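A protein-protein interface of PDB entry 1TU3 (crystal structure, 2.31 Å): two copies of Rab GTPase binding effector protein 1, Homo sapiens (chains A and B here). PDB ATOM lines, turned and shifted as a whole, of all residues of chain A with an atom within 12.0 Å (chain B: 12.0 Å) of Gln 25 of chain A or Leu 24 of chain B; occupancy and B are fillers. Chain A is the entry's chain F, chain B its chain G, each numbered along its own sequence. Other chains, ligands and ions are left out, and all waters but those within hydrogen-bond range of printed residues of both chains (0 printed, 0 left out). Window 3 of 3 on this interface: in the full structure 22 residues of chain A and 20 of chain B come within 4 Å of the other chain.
The side-chain amide nitrogen (NE2) of Gln 35 of chain B lies within hydrogen-bond range of the backbone carbonyl oxygen (O) of Ser 31 of chain A (3.0 Å).
OG of Ser 31 of chain A lies within hydrogen-bond range of OE2 of Glu 32 of chain B (2.9 Å).
The side-chain hydroxyl (OG) of Ser 31 of chain A lies within hydrogen-bond range of the side-chain hydroxyl (OG) of Ser 31 of chain B, at 2.7 Å.
The backbone carbonyl oxygen of Ser 31 of chain B is in hydrogen-bond range of the side-chain amide nitrogen of Gln 35 of chain A (3.1 Å).
Hydrophobic or aromatic side chains of chain B within 4 Å of the printed part of chain A: Leu 24 and Leu 28.
Of the 16 printed residues of chain A, 8 touch a printed residue of chain B.
Along chain A the printed residues that touch a printed residue of chain B span positions 24 to 35.
Among the printed residues, 14 pairs touch across the chains.
Among the printed residues, no Asp or Glu carboxylate lies within 4 Å of a Lys or Arg side-chain nitrogen of the other chain.
CD2 of Leu 24 of chain A touches CD2 of Leu 24 of chain B, 3.3 Å away.
CD2 of Leu 24 of chain A touches NE2 of Gln 25 of chain B, 3.3 Å away.
Gln 25 of chain A touches Leu 24 of chain B (OE1 to CD1, 3.2 Å).
OE1 of Glu 27 of chain A touches CD2 of Leu 28 of chain B, 3.0 Å away.
Leu 28 of chain A touches Glu 27 of chain B.
Leu 28 of chain A touches Leu 28 of chain B (CD1 to CA, 3.5 Å).
Glu 32 of chain A touches Glu 27 of chain B (OE2 to OE2, 3.8 Å).
Glu 32 of chain A touches Ser 31 of chain B (CG to OG, 3.4 Å).
Gln 35 of chain B touches Val 34 of chain A.
Gln 35 of chain A touches Gln 35 of chain B.
Leu 24 of chain A touches Gln 25 of chain B, and with the chains exchanged Gln 25 of chain A touches Leu 24 of chain B.
Leu 28 of chain A touches its own counterpart, Leu 28 of chain B.
Ser 31 of chain A touches Glu 32 of chain B, and with the chains exchanged Glu 32 of chain A touches Ser 31 of chain B.
Gln 35 of chain B touches its own counterpart, Gln 35 of chain A.
Leu 24 of chain B touches just these residues of chain A: Leu 24 (3.3 Å) and Gln 25 (3.2 Å).
No residue of chain B comes within 4 Å of Ala 21 of chain A.
No residue of chain B comes within 4 Å of Gln 22 of chain A.
No residue of chain B comes within 4 Å of Arg 23 of chain A.
Leu 24 of chain A touches just these residues of chain B: Leu 24 (3.3 Å) and Gln 25 (3.3 Å).
Thr 26 of chain A touches none of the printed residues of chain B.
Of chain B, only Leu 28 comes within 4 Å of Glu 27 of chain A.
Of chain B, only Glu 27 (3.3 Å) and Leu 28 (3.5 Å) come within 4 Å of Leu 28 of chain A.
No residue of chain B comes within 4 Å of Asp 29 of chain A.
No residue of chain A comes within 4 Å of Lys 20 of chain B.
No residue of chain A comes within 4 Å of Ala 21 of chain B.
No residue of chain A comes within 4 Å of Arg 23 of chain B.
Of chain A, only Leu 28 and Glu 32 come within 4 Å of Glu 27 of chain B.
Printed residues of chain A within 4 Å of Glu 32 of chain B: Ser 31.
Of the printed residues of chain B, Glu 32 of chain A touches Glu 27 and Ser 31.
Asn 19 of chain B touches none of the printed residues of chain A.
Val 30 of chain B touches none of the printed residues of chain A.
The nearest residue of chain A that does not touch Leu 24 of chain B is Leu 28 of chain A (4.7 Å).
The nearest printed residue of chain B that does not touch Glu 32 of chain A is Gln 35 of chain B (5.0 Å).
The side-chain carboxylate (OD2) of Asp 29 of chain B sits close to the backbone carbonyl oxygen (O) of Gln 25 of chain B (2.6 Å).
The side-chain carboxylate (OD1) of Asp 29 of chain A is in hydrogen-bond range of the side-chain amide nitrogen (NE2) of Gln 25 of chain A (3.3 Å).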
ATOM      1  N   ALA A  21       9.862   8.467  16.283  1.00  0.00           N
ATOM      2  CA  ALA A  21      10.492   7.317  15.572  1.00  0.00           C
ATOM      3  C   ALA A  21      11.698   7.765  14.738  1.00  0.00           C
ATOM      4  O   ALA A  21      12.221   8.863  14.919  1.00  0.00           O
ATOM      5  CB  ALA A  21       9.448   6.625  14.678  1.00  0.00           C
ATOM      6  N   GLN A  22      12.137   6.894  13.836  1.00  0.00           N
ATOM      7  CA  GLN A  22      13.201   7.207  12.883  1.00  0.00           C
ATOM      8  C   GLN A  22      12.700   8.219  11.855  1.00  0.00           C
ATOM      9  O   GLN A  22      13.448   9.091  11.405  1.00  0.00           O
ATOM     10  CB  GLN A  22      13.636   5.922  12.169  1.00  0.00           C
ATOM     11  CG  GLN A  22      14.543   6.116  10.957  1.00  0.00           C
ATOM     12  CD  GLN A  22      15.996   6.321  11.327  1.00  0.00           C
ATOM     13  OE1 GLN A  22      16.873   6.323  10.460  1.00  0.00           O
ATOM     14  NE2 GLN A  22      16.263   6.494  12.620  1.00  0.00           N
ATOM     15  N   ARG A  23      11.428   8.091  11.488  1.00  0.00           N
ATOM     16  CA  ARG A  23      10.850   8.905  10.428  1.00  0.00           C
ATOM     17  C   ARG A  23      10.505  10.289  10.963  1.00  0.00           C
ATOM     18  O   ARG A  23      10.601  11.282  10.245  1.00  0.00           O
ATOM     19  CB  ARG A  23       9.598   8.214   9.850  1.00  0.00           C
ATOM     20  CG  ARG A  23       8.340   8.249  10.727  1.00  0.00           C
ATOM     21  CD  ARG A  23       7.519   9.520  10.478  1.00  0.00           C
ATOM     22  NE  ARG A  23       6.220   9.506  11.156  1.00  0.00           N
ATOM     23  CZ  ARG A  23       6.053   9.533  12.477  1.00  0.00           C
ATOM     24  NH1 ARG A  23       7.109   9.575  13.281  1.00  0.00           N
ATOM     25  NH2 ARG A  23       4.829   9.525  12.995  1.00  0.00           N
ATOM     26  N   LEU A  24      10.116  10.343  12.231  1.00  0.00           N
ATOM     27  CA  LEU A  24       9.759  11.598  12.863  1.00  0.00           C
ATOM     28  C   LEU A  24      10.974  12.523  12.863  1.00  0.00           C
ATOM     29  O   LEU A  24      10.834  13.745  12.760  1.00  0.00           O
ATOM     30  CB  LEU A  24       9.300  11.344  14.295  1.00  0.00           C
ATOM     31  CG  LEU A  24       8.161  12.212  14.838  1.00  0.00           C
ATOM     32  CD1 LEU A  24       7.972  11.913  16.325  1.00  0.00           C
ATOM     33  CD2 LEU A  24       8.464  13.686  14.627  1.00  0.00           C
ATOM     34  N   GLN A  25      12.163  11.927  12.975  1.00  0.00           N
ATOM     35  CA  GLN A  25      13.419  12.674  12.968  1.00  0.00           C
ATOM     36  C   GLN A  25      13.731  13.216  11.582  1.00  0.00           C
ATOM     37  O   GLN A  25      14.205  14.345  11.442  1.00  0.00           O
ATOM     38  CB  GLN A  25      14.589  11.786  13.416  1.00  0.00           C
ATOM     39  CG  GLN A  25      15.937  12.509  13.515  1.00  0.00           C
ATOM     40  CD  GLN A  25      15.940  13.615  14.569  1.00  0.00           C
ATOM     41  OE1 GLN A  25      15.535  13.391  15.715  1.00  0.00           O
ATOM     42  NE2 GLN A  25      16.403  14.817  14.187  1.00  0.00           N
ATOM     43  N   THR A  26      13.485  12.388  10.569  1.00  0.00           N
ATOM     44  CA  THR A  26      13.742  12.758   9.182  1.00  0.00           C
ATOM     45  C   THR A  26      12.680  13.761   8.737  1.00  0.00           C
ATOM     46  O   THR A  26      12.942  14.641   7.917  1.00  0.00           O
ATOM     47  CB  THR A  26      13.674  11.535   8.250  1.00  0.00           C
ATOM     48  OG1 THR A  26      12.327  11.055   8.207  1.00  0.00           O
ATOM     49  CG2 THR A  26      14.565  10.425   8.762  1.00  0.00           C
ATOM     50  N   GLU A  27      11.477  13.614   9.288  1.00  0.00           N
ATOM     51  CA  GLU A  27      10.412  14.581   9.059  1.00  0.00           C
ATOM     52  C   GLU A  27      10.852  15.955   9.573  1.00  0.00           C
ATOM     53  O   GLU A  27      10.748  16.954   8.858  1.00  0.00           O
ATOM     54  CB  GLU A  27       9.139  14.142   9.777  1.00  0.00           C
ATOM     55  CG  GLU A  27       8.004  15.155   9.745  1.00  0.00           C
ATOM     56  CD  GLU A  27       6.942  14.841  10.784  1.00  0.00           C
ATOM     57  OE1 GLU A  27       7.321  14.627  11.956  1.00  0.00           O
ATOM     58  OE2 GLU A  27       5.739  14.807  10.435  1.00  0.00           O
ATOM     59  N   LEU A  28      11.341  15.996  10.813  1.00  0.00           N
ATOM     60  CA  LEU A  28      11.877  17.225  11.392  1.00  0.00           C
ATOM     61  C   LEU A  28      12.968  17.841  10.513  1.00  0.00           C
ATOM     62  O   LEU A  28      12.935  19.030  10.214  1.00  0.00           O
ATOM     63  CB  LEU A  28      12.441  16.960  12.784  1.00  0.00           C
ATOM     64  CG  LEU A  28      13.044  18.148  13.534  1.00  0.00           C
ATOM     65  CD1 LEU A  28      11.969  19.142  13.938  1.00  0.00           C
ATOM     66  CD2 LEU A  28      13.748  17.631  14.769  1.00  0.00           C
ATOM     67  N   ASP A  29      13.929  17.033  10.091  1.00  0.00           N
ATOM     68  CA  ASP A  29      15.020  17.539   9.276  1.00  0.00           C
ATOM     69  C   ASP A  29      14.522  18.240   8.018  1.00  0.00           C
ATOM     70  O   ASP A  29      14.923  19.369   7.737  1.00  0.00           O
ATOM     71  CB  ASP A  29      15.977  16.404   8.920  1.00  0.00           C
ATOM     72  CG  ASP A  29      16.536  15.701  10.166  1.00  0.00           C
ATOM     73  OD1 ASP A  29      16.623  16.369  11.229  1.00  0.00           O
ATOM     74  OD2 ASP A  29      16.892  14.494  10.083  1.00  0.00           O
ATOM     75  N   VAL A  30      13.642  17.579   7.273  1.00  0.00           N
ATOM     76  CA  VAL A  30      13.059  18.150   6.062  1.00  0.00           C
ATOM     77  C   VAL A  30      12.345  19.478   6.352  1.00  0.00           C
ATOM     78  O   VAL A  30      12.500  20.463   5.622  1.00  0.00           O
ATOM     79  CB  VAL A  30      12.052  17.166   5.431  1.00  0.00           C
ATOM     80  CG1 VAL A  30      11.272  17.846   4.302  1.00  0.00           C
ATOM     81  CG2 VAL A  30      12.813  15.955   4.894  1.00  0.00           C
ATOM     82  N   SER A  31      11.577  19.470   7.433  1.00  0.00           N
ATOM     83  CA  SER A  31      10.863  20.621   7.933  1.00  0.00           C
ATOM     84  C   SER A  31      11.824  21.802   8.088  1.00  0.00           C
ATOM     85  O   SER A  31      11.594  22.895   7.562  1.00  0.00           O
ATOM     86  CB  SER A  31      10.251  20.263   9.294  1.00  0.00           C
ATOM     87  OG  SER A  31       9.559  21.343   9.890  1.00  0.00           O
ATOM     88  N   GLU A  32      12.906  21.565   8.822  1.00  0.00           N
ATOM     89  CA  GLU A  32      13.822  22.624   9.190  1.00  0.00           C
ATOM     90  C   GLU A  32      14.638  23.070   7.975  1.00  0.00           C
ATOM     91  O   GLU A  32      15.117  24.194   7.920  1.00  0.00           O
ATOM     92  CB  GLU A  32      14.732  22.152  10.316  1.00  0.00           C
ATOM     93  CG  GLU A  32      14.082  22.157  11.686  1.00  0.00           C
ATOM     94  CD  GLU A  32      15.104  22.000  12.799  1.00  0.00           C
ATOM     95  OE1 GLU A  32      16.148  22.689  12.738  1.00  0.00           O
ATOM     96  OE2 GLU A  32      14.871  21.199  13.731  1.00  0.00           O
ATOM     97  N   GLN A  33      14.770  22.181   6.998  1.00  0.00           N
ATOM     98  CA  GLN A  33      15.468  22.483   5.757  1.00  0.00           C
ATOM     99  C   GLN A  33      14.639  23.505   4.948  1.00  0.00           C
ATOM    100  O   GLN A  33      15.185  24.481   4.453  1.00  0.00           O
ATOM    101  CB  GLN A  33      15.658  21.187   4.951  1.00  0.00           C
ATOM    102  CG  GLN A  33      16.663  21.248   3.798  1.00  0.00           C
ATOM    103  CD  GLN A  33      16.527  20.046   2.848  1.00  0.00           C
ATOM    104  OE1 GLN A  33      16.221  18.932   3.275  1.00  0.00           O
ATOM    105  NE2 GLN A  33      16.758  20.274   1.559  1.00  0.00           N
ATOM    106  N   VAL A  34      13.328  23.267   4.841  1.00  0.00           N
ATOM    107  CA  VAL A  34      12.404  24.159   4.139  1.00  0.00           C
ATOM    108  C   VAL A  34      12.337  25.499   4.901  1.00  0.00           C
ATOM    109  O   VAL A  34      12.445  26.588   4.311  1.00  0.00           O
ATOM    110  CB  VAL A  34      10.981  23.510   4.033  1.00  0.00           C
ATOM    111  CG1 VAL A  34      10.015  24.393   3.246  1.00  0.00           C
ATOM    112  CG2 VAL A  34      11.097  22.151   3.328  1.00  0.00           C
ATOM    113  N   GLN A  35      12.191  25.400   6.217  1.00  0.00           N
ATOM    114  CA  GLN A  35      12.185  26.566   7.078  1.00  0.00           C
ATOM    115  C   GLN A  35      13.368  27.478   6.753  1.00  0.00           C
ATOM    116  O   GLN A  35      13.232  28.707   6.727  1.00  0.00           O
ATOM    117  CB  GLN A  35      12.221  26.130   8.554  1.00  0.00           C
ATOM    118  CG  GLN A  35      12.627  27.203   9.485  1.00  0.00           C
ATOM    119  CD  GLN A  35      12.770  26.735  10.928  1.00  0.00           C
ATOM    120  OE1 GLN A  35      13.715  27.108  11.613  1.00  0.00           O
ATOM    121  NE2 GLN A  35      11.818  25.959  11.404  1.00  0.00           N
ATOM    122  N   ARG A  36      14.527  26.878   6.495  1.00  0.00           N
ATOM    123  CA  ARG A  36      15.720  27.659   6.214  1.00  0.00           C
ATOM    124  C   ARG A  36      15.730  28.160   4.777  1.00  0.00           C
ATOM    125  O   ARG A  36      16.269  29.233   4.487  1.00  0.00           O
ATOM    126  CB  ARG A  36      16.984  26.844   6.538  1.00  0.00           C
ATOM    127  CG  ARG A  36      17.131  26.738   8.034  1.00  0.00           C
ATOM    128  CD  ARG A  36      18.487  26.303   8.538  1.00  0.00           C
ATOM    129  NE  ARG A  36      18.624  24.874   8.360  1.00  0.00           N
ATOM    130  CZ  ARG A  36      19.028  24.323   7.234  1.00  0.00           C
ATOM    131  NH1 ARG A  36      19.354  25.112   6.221  1.00  0.00           N
ATOM    132  NH2 ARG A  36      19.021  23.003   7.099  1.00  0.00           N
ATOM    133  N   ASN B  19       9.572  10.197  26.094  1.00  0.00           N
ATOM    134  CA  ASN B  19      10.668  11.159  26.399  1.00  0.00           C
ATOM    135  C   ASN B  19      11.419  11.553  25.128  1.00  0.00           C
ATOM    136  O   ASN B  19      11.740  12.731  24.922  1.00  0.00           O
ATOM    137  CB  ASN B  19      11.636  10.541  27.419  1.00  0.00           C
ATOM    138  CG  ASN B  19      11.109  10.614  28.853  1.00  0.00           C
ATOM    139  OD1 ASN B  19       9.971  10.225  29.137  1.00  0.00           O
ATOM    140  ND2 ASN B  19      11.945  11.110  29.765  1.00  0.00           N
ATOM    141  N   LYS B  20      11.685  10.562  24.278  1.00  0.00           N
ATOM    142  CA  LYS B  20      12.405  10.790  23.027  1.00  0.00           C
ATOM    143  C   LYS B  20      11.467  11.366  21.967  1.00  0.00           C
ATOM    144  O   LYS B  20      11.618  12.515  21.549  1.00  0.00           O
ATOM    145  CB  LYS B  20      13.026   9.475  22.520  1.00  0.00           C
ATOM    146  CG  LYS B  20      13.828   9.619  21.224  1.00  0.00           C
ATOM    147  CD  LYS B  20      14.386   8.282  20.721  1.00  0.00           C
ATOM    148  CE  LYS B  20      15.623   7.842  21.488  1.00  0.00           C
ATOM    149  NZ  LYS B  20      16.768   8.774  21.275  1.00  0.00           N
ATOM    150  N   ALA B  21      10.494  10.565  21.541  1.00  0.00           N
ATOM    151  CA  ALA B  21       9.545  10.994  20.522  1.00  0.00           C
ATOM    152  C   ALA B  21       8.578  12.045  21.061  1.00  0.00           C
ATOM    153  O   ALA B  21       7.681  12.493  20.347  1.00  0.00           O
ATOM    154  CB  ALA B  21       8.767   9.797  20.001  1.00  0.00           C
ATOM    155  N   GLN B  22       8.757  12.427  22.322  1.00  0.00           N
ATOM    156  CA  GLN B  22       7.892  13.423  22.940  1.00  0.00           C
ATOM    157  C   GLN B  22       8.355  14.798  22.504  1.00  0.00           C
ATOM    158  O   GLN B  22       7.774  15.414  21.605  1.00  0.00           O
ATOM    159  CB  GLN B  22       7.951  13.337  24.474  1.00  0.00           C
ATOM    160  CG  GLN B  22       7.478  12.016  25.073  1.00  0.00           C
ATOM    161  CD  GLN B  22       7.325  12.072  26.591  1.00  0.00           C
ATOM    162  OE1 GLN B  22       8.234  12.491  27.310  1.00  0.00           O
ATOM    163  NE2 GLN B  22       6.169  11.638  27.083  1.00  0.00           N
ATOM    164  N   ARG B  23       9.418  15.266  23.149  1.00  0.00           N
ATOM    165  CA  ARG B  23       9.949  16.599  22.914  1.00  0.00           C
ATOM    166  C   ARG B  23      10.305  16.788  21.435  1.00  0.00           C
ATOM    167  O   ARG B  23      10.559  17.907  20.981  1.00  0.00           O
ATOM    168  CB  ARG B  23      11.184  16.819  23.800  1.00  0.00           C
ATOM    169  CG  ARG B  23      10.961  16.427  25.266  1.00  0.00           C
ATOM    170  CD  ARG B  23      12.056  16.942  26.211  1.00  0.00           C
ATOM    171  NE  ARG B  23      13.316  16.195  26.150  1.00  0.00           N
ATOM    172  CZ  ARG B  23      14.270  16.374  25.239  1.00  0.00           C
ATOM    173  NH1 ARG B  23      14.127  17.284  24.283  1.00  0.00           N
ATOM    174  NH2 ARG B  23      15.383  15.646  25.294  1.00  0.00           N
ATOM    175  N   LEU B  24      10.307  15.688  20.690  1.00  0.00           N
ATOM    176  CA  LEU B  24      10.683  15.714  19.288  1.00  0.00           C
ATOM    177  C   LEU B  24       9.471  16.061  18.426  1.00  0.00           C
ATOM    178  O   LEU B  24       9.604  16.704  17.384  1.00  0.00           O
ATOM    179  CB  LEU B  24      11.257  14.351  18.891  1.00  0.00           C
ATOM    180  CG  LEU B  24      12.081  14.224  17.607  1.00  0.00           C
ATOM    181  CD1 LEU B  24      13.122  13.144  17.808  1.00  0.00           C
ATOM    182  CD2 LEU B  24      11.197  13.903  16.417  1.00  0.00           C
ATOM    183  N   GLN B  25       8.287  15.641  18.863  1.00  0.00           N
ATOM    184  CA  GLN B  25       7.058  15.992  18.156  1.00  0.00           C
ATOM    185  C   GLN B  25       6.811  17.484  18.257  1.00  0.00           C
ATOM    186  O   GLN B  25       6.414  18.125  17.282  1.00  0.00           O
ATOM    187  CB  GLN B  25       5.859  15.251  18.743  1.00  0.00           C
ATOM    188  CG  GLN B  25       5.362  14.085  17.902  1.00  0.00           C
ATOM    189  CD  GLN B  25       4.860  14.510  16.532  1.00  0.00           C
ATOM    190  OE1 GLN B  25       4.126  15.491  16.404  1.00  0.00           O
ATOM    191  NE2 GLN B  25       5.242  13.760  15.500  1.00  0.00           N
ATOM    192  N   THR B  26       7.047  18.024  19.449  1.00  0.00           N
ATOM    193  CA  THR B  26       6.873  19.448  19.691  1.00  0.00           C
ATOM    194  C   THR B  26       7.884  20.280  18.892  1.00  0.00           C
ATOM    195  O   THR B  26       7.519  21.250  18.224  1.00  0.00           O
ATOM    196  CB  THR B  26       7.030  19.768  21.184  1.00  0.00           C
ATOM    197  OG1 THR B  26       8.334  19.362  21.621  1.00  0.00           O
ATOM    198  CG2 THR B  26       5.972  19.038  21.993  1.00  0.00           C
ATOM    199  N   GLU B  27       9.156  19.897  18.968  1.00  0.00           N
ATOM    200  CA  GLU B  27      10.200  20.567  18.214  1.00  0.00           C
ATOM    201  C   GLU B  27       9.853  20.664  16.726  1.00  0.00           C
ATOM    202  O   GLU B  27      10.205  21.639  16.061  1.00  0.00           O
ATOM    203  CB  GLU B  27      11.520  19.826  18.382  1.00  0.00           C
ATOM    204  CG  GLU B  27      12.673  20.499  17.700  1.00  0.00           C
ATOM    205  CD  GLU B  27      14.002  19.915  18.107  1.00  0.00           C
ATOM    206  OE1 GLU B  27      14.244  19.792  19.326  1.00  0.00           O
ATOM    207  OE2 GLU B  27      14.808  19.584  17.209  1.00  0.00           O
ATOM    208  N   LEU B  28       9.171  19.644  16.212  1.00  0.00           N
ATOM    209  CA  LEU B  28       8.642  19.658  14.855  1.00  0.00           C
ATOM    210  C   LEU B  28       7.549  20.712  14.673  1.00  0.00           C
ATOM    211  O   LEU B  28       7.542  21.451  13.697  1.00  0.00           O
ATOM    212  CB  LEU B  28       8.065  18.299  14.513  1.00  0.00           C
ATOM    213  CG  LEU B  28       7.256  18.215  13.232  1.00  0.00           C
ATOM    214  CD1 LEU B  28       8.167  18.044  12.016  1.00  0.00           C
ATOM    215  CD2 LEU B  28       6.309  17.033  13.364  1.00  0.00           C
ATOM    216  N   ASP B  29       6.617  20.761  15.611  1.00  0.00           N
ATOM    217  CA  ASP B  29       5.465  21.634  15.471  1.00  0.00           C
ATOM    218  C   ASP B  29       5.878  23.093  15.499  1.00  0.00           C
ATOM    219  O   ASP B  29       5.306  23.917  14.786  1.00  0.00           O
ATOM    220  CB  ASP B  29       4.457  21.351  16.582  1.00  0.00           C
ATOM    221  CG  ASP B  29       3.971  19.907  16.571  1.00  0.00           C
ATOM    222  OD1 ASP B  29       3.483  19.451  15.509  1.00  0.00           O
ATOM    223  OD2 ASP B  29       4.077  19.233  17.622  1.00  0.00           O
ATOM    224  N   VAL B  30       6.879  23.400  16.318  1.00  0.00           N
ATOM    225  CA  VAL B  30       7.399  24.755  16.428  1.00  0.00           C
ATOM    226  C   VAL B  30       8.127  25.082  15.125  1.00  0.00           C
ATOM    227  O   VAL B  30       7.984  26.161  14.554  1.00  0.00           O
ATOM    228  CB  VAL B  30       8.361  24.868  17.640  1.00  0.00           C
ATOM    229  CG1 VAL B  30       9.121  26.191  17.628  1.00  0.00           C
ATOM    230  CG2 VAL B  30       7.555  24.753  18.916  1.00  0.00           C
ATOM    231  N   SER B  31       8.892  24.117  14.653  1.00  0.00           N
ATOM    232  CA  SER B  31       9.528  24.204  13.374  1.00  0.00           C
ATOM    233  C   SER B  31       8.504  24.566  12.288  1.00  0.00           C
ATOM    234  O   SER B  31       8.704  25.517  11.537  1.00  0.00           O
ATOM    235  CB  SER B  31      10.214  22.862  13.072  1.00  0.00           C
ATOM    236  OG  SER B  31      10.746  22.831  11.774  1.00  0.00           O
ATOM    237  N   GLU B  32       7.407  23.819  12.213  1.00  0.00           N
ATOM    238  CA  GLU B  32       6.375  24.046  11.201  1.00  0.00           C
ATOM    239  C   GLU B  32       5.752  25.425  11.377  1.00  0.00           C
ATOM    240  O   GLU B  32       5.397  26.098  10.411  1.00  0.00           O
ATOM    241  CB  GLU B  32       5.283  22.983  11.311  1.00  0.00           C
ATOM    242  CG  GLU B  32       5.739  21.559  10.991  1.00  0.00           C
ATOM    243  CD  GLU B  32       5.726  21.250   9.507  1.00  0.00           C
ATOM    244  OE1 GLU B  32       4.622  21.057   8.947  1.00  0.00           O
ATOM    245  OE2 GLU B  32       6.820  21.200   8.901  1.00  0.00           O
ATOM    246  N   GLN B  33       5.631  25.854  12.618  1.00  0.00           N
ATOM    247  CA  GLN B  33       5.058  27.153  12.876  1.00  0.00           C
ATOM    248  C   GLN B  33       5.982  28.284  12.357  1.00  0.00           C
ATOM    249  O   GLN B  33       5.509  29.272  11.797  1.00  0.00           O
ATOM    250  CB  GLN B  33       4.820  27.305  14.373  1.00  0.00           C
ATOM    251  CG  GLN B  33       4.126  28.566  14.747  1.00  0.00           C
ATOM    252  CD  GLN B  33       4.090  28.733  16.235  1.00  0.00           C
ATOM    253  OE1 GLN B  33       3.836  27.769  16.967  1.00  0.00           O
ATOM    254  NE2 GLN B  33       4.343  29.958  16.705  1.00  0.00           N
ATOM    255  N   GLN B  35       8.221  27.954  10.029  1.00  0.00           N
ATOM    256  CA  GLN B  35       8.246  27.770   8.614  1.00  0.00           C
ATOM    257  C   GLN B  35       7.156  28.597   7.941  1.00  0.00           C
ATOM    258  O   GLN B  35       7.410  29.308   6.967  1.00  0.00           O
ATOM    259  CB  GLN B  35       8.024  26.317   8.317  1.00  0.00           C
ATOM    260  CG  GLN B  35       8.244  25.967   6.901  1.00  0.00           C
ATOM    261  CD  GLN B  35       7.866  24.541   6.651  1.00  0.00           C
ATOM    262  OE1 GLN B  35       6.701  24.232   6.450  1.00  0.00           O
ATOM    263  NE2 GLN B  35       8.845  23.656   6.690  1.00  0.00           N
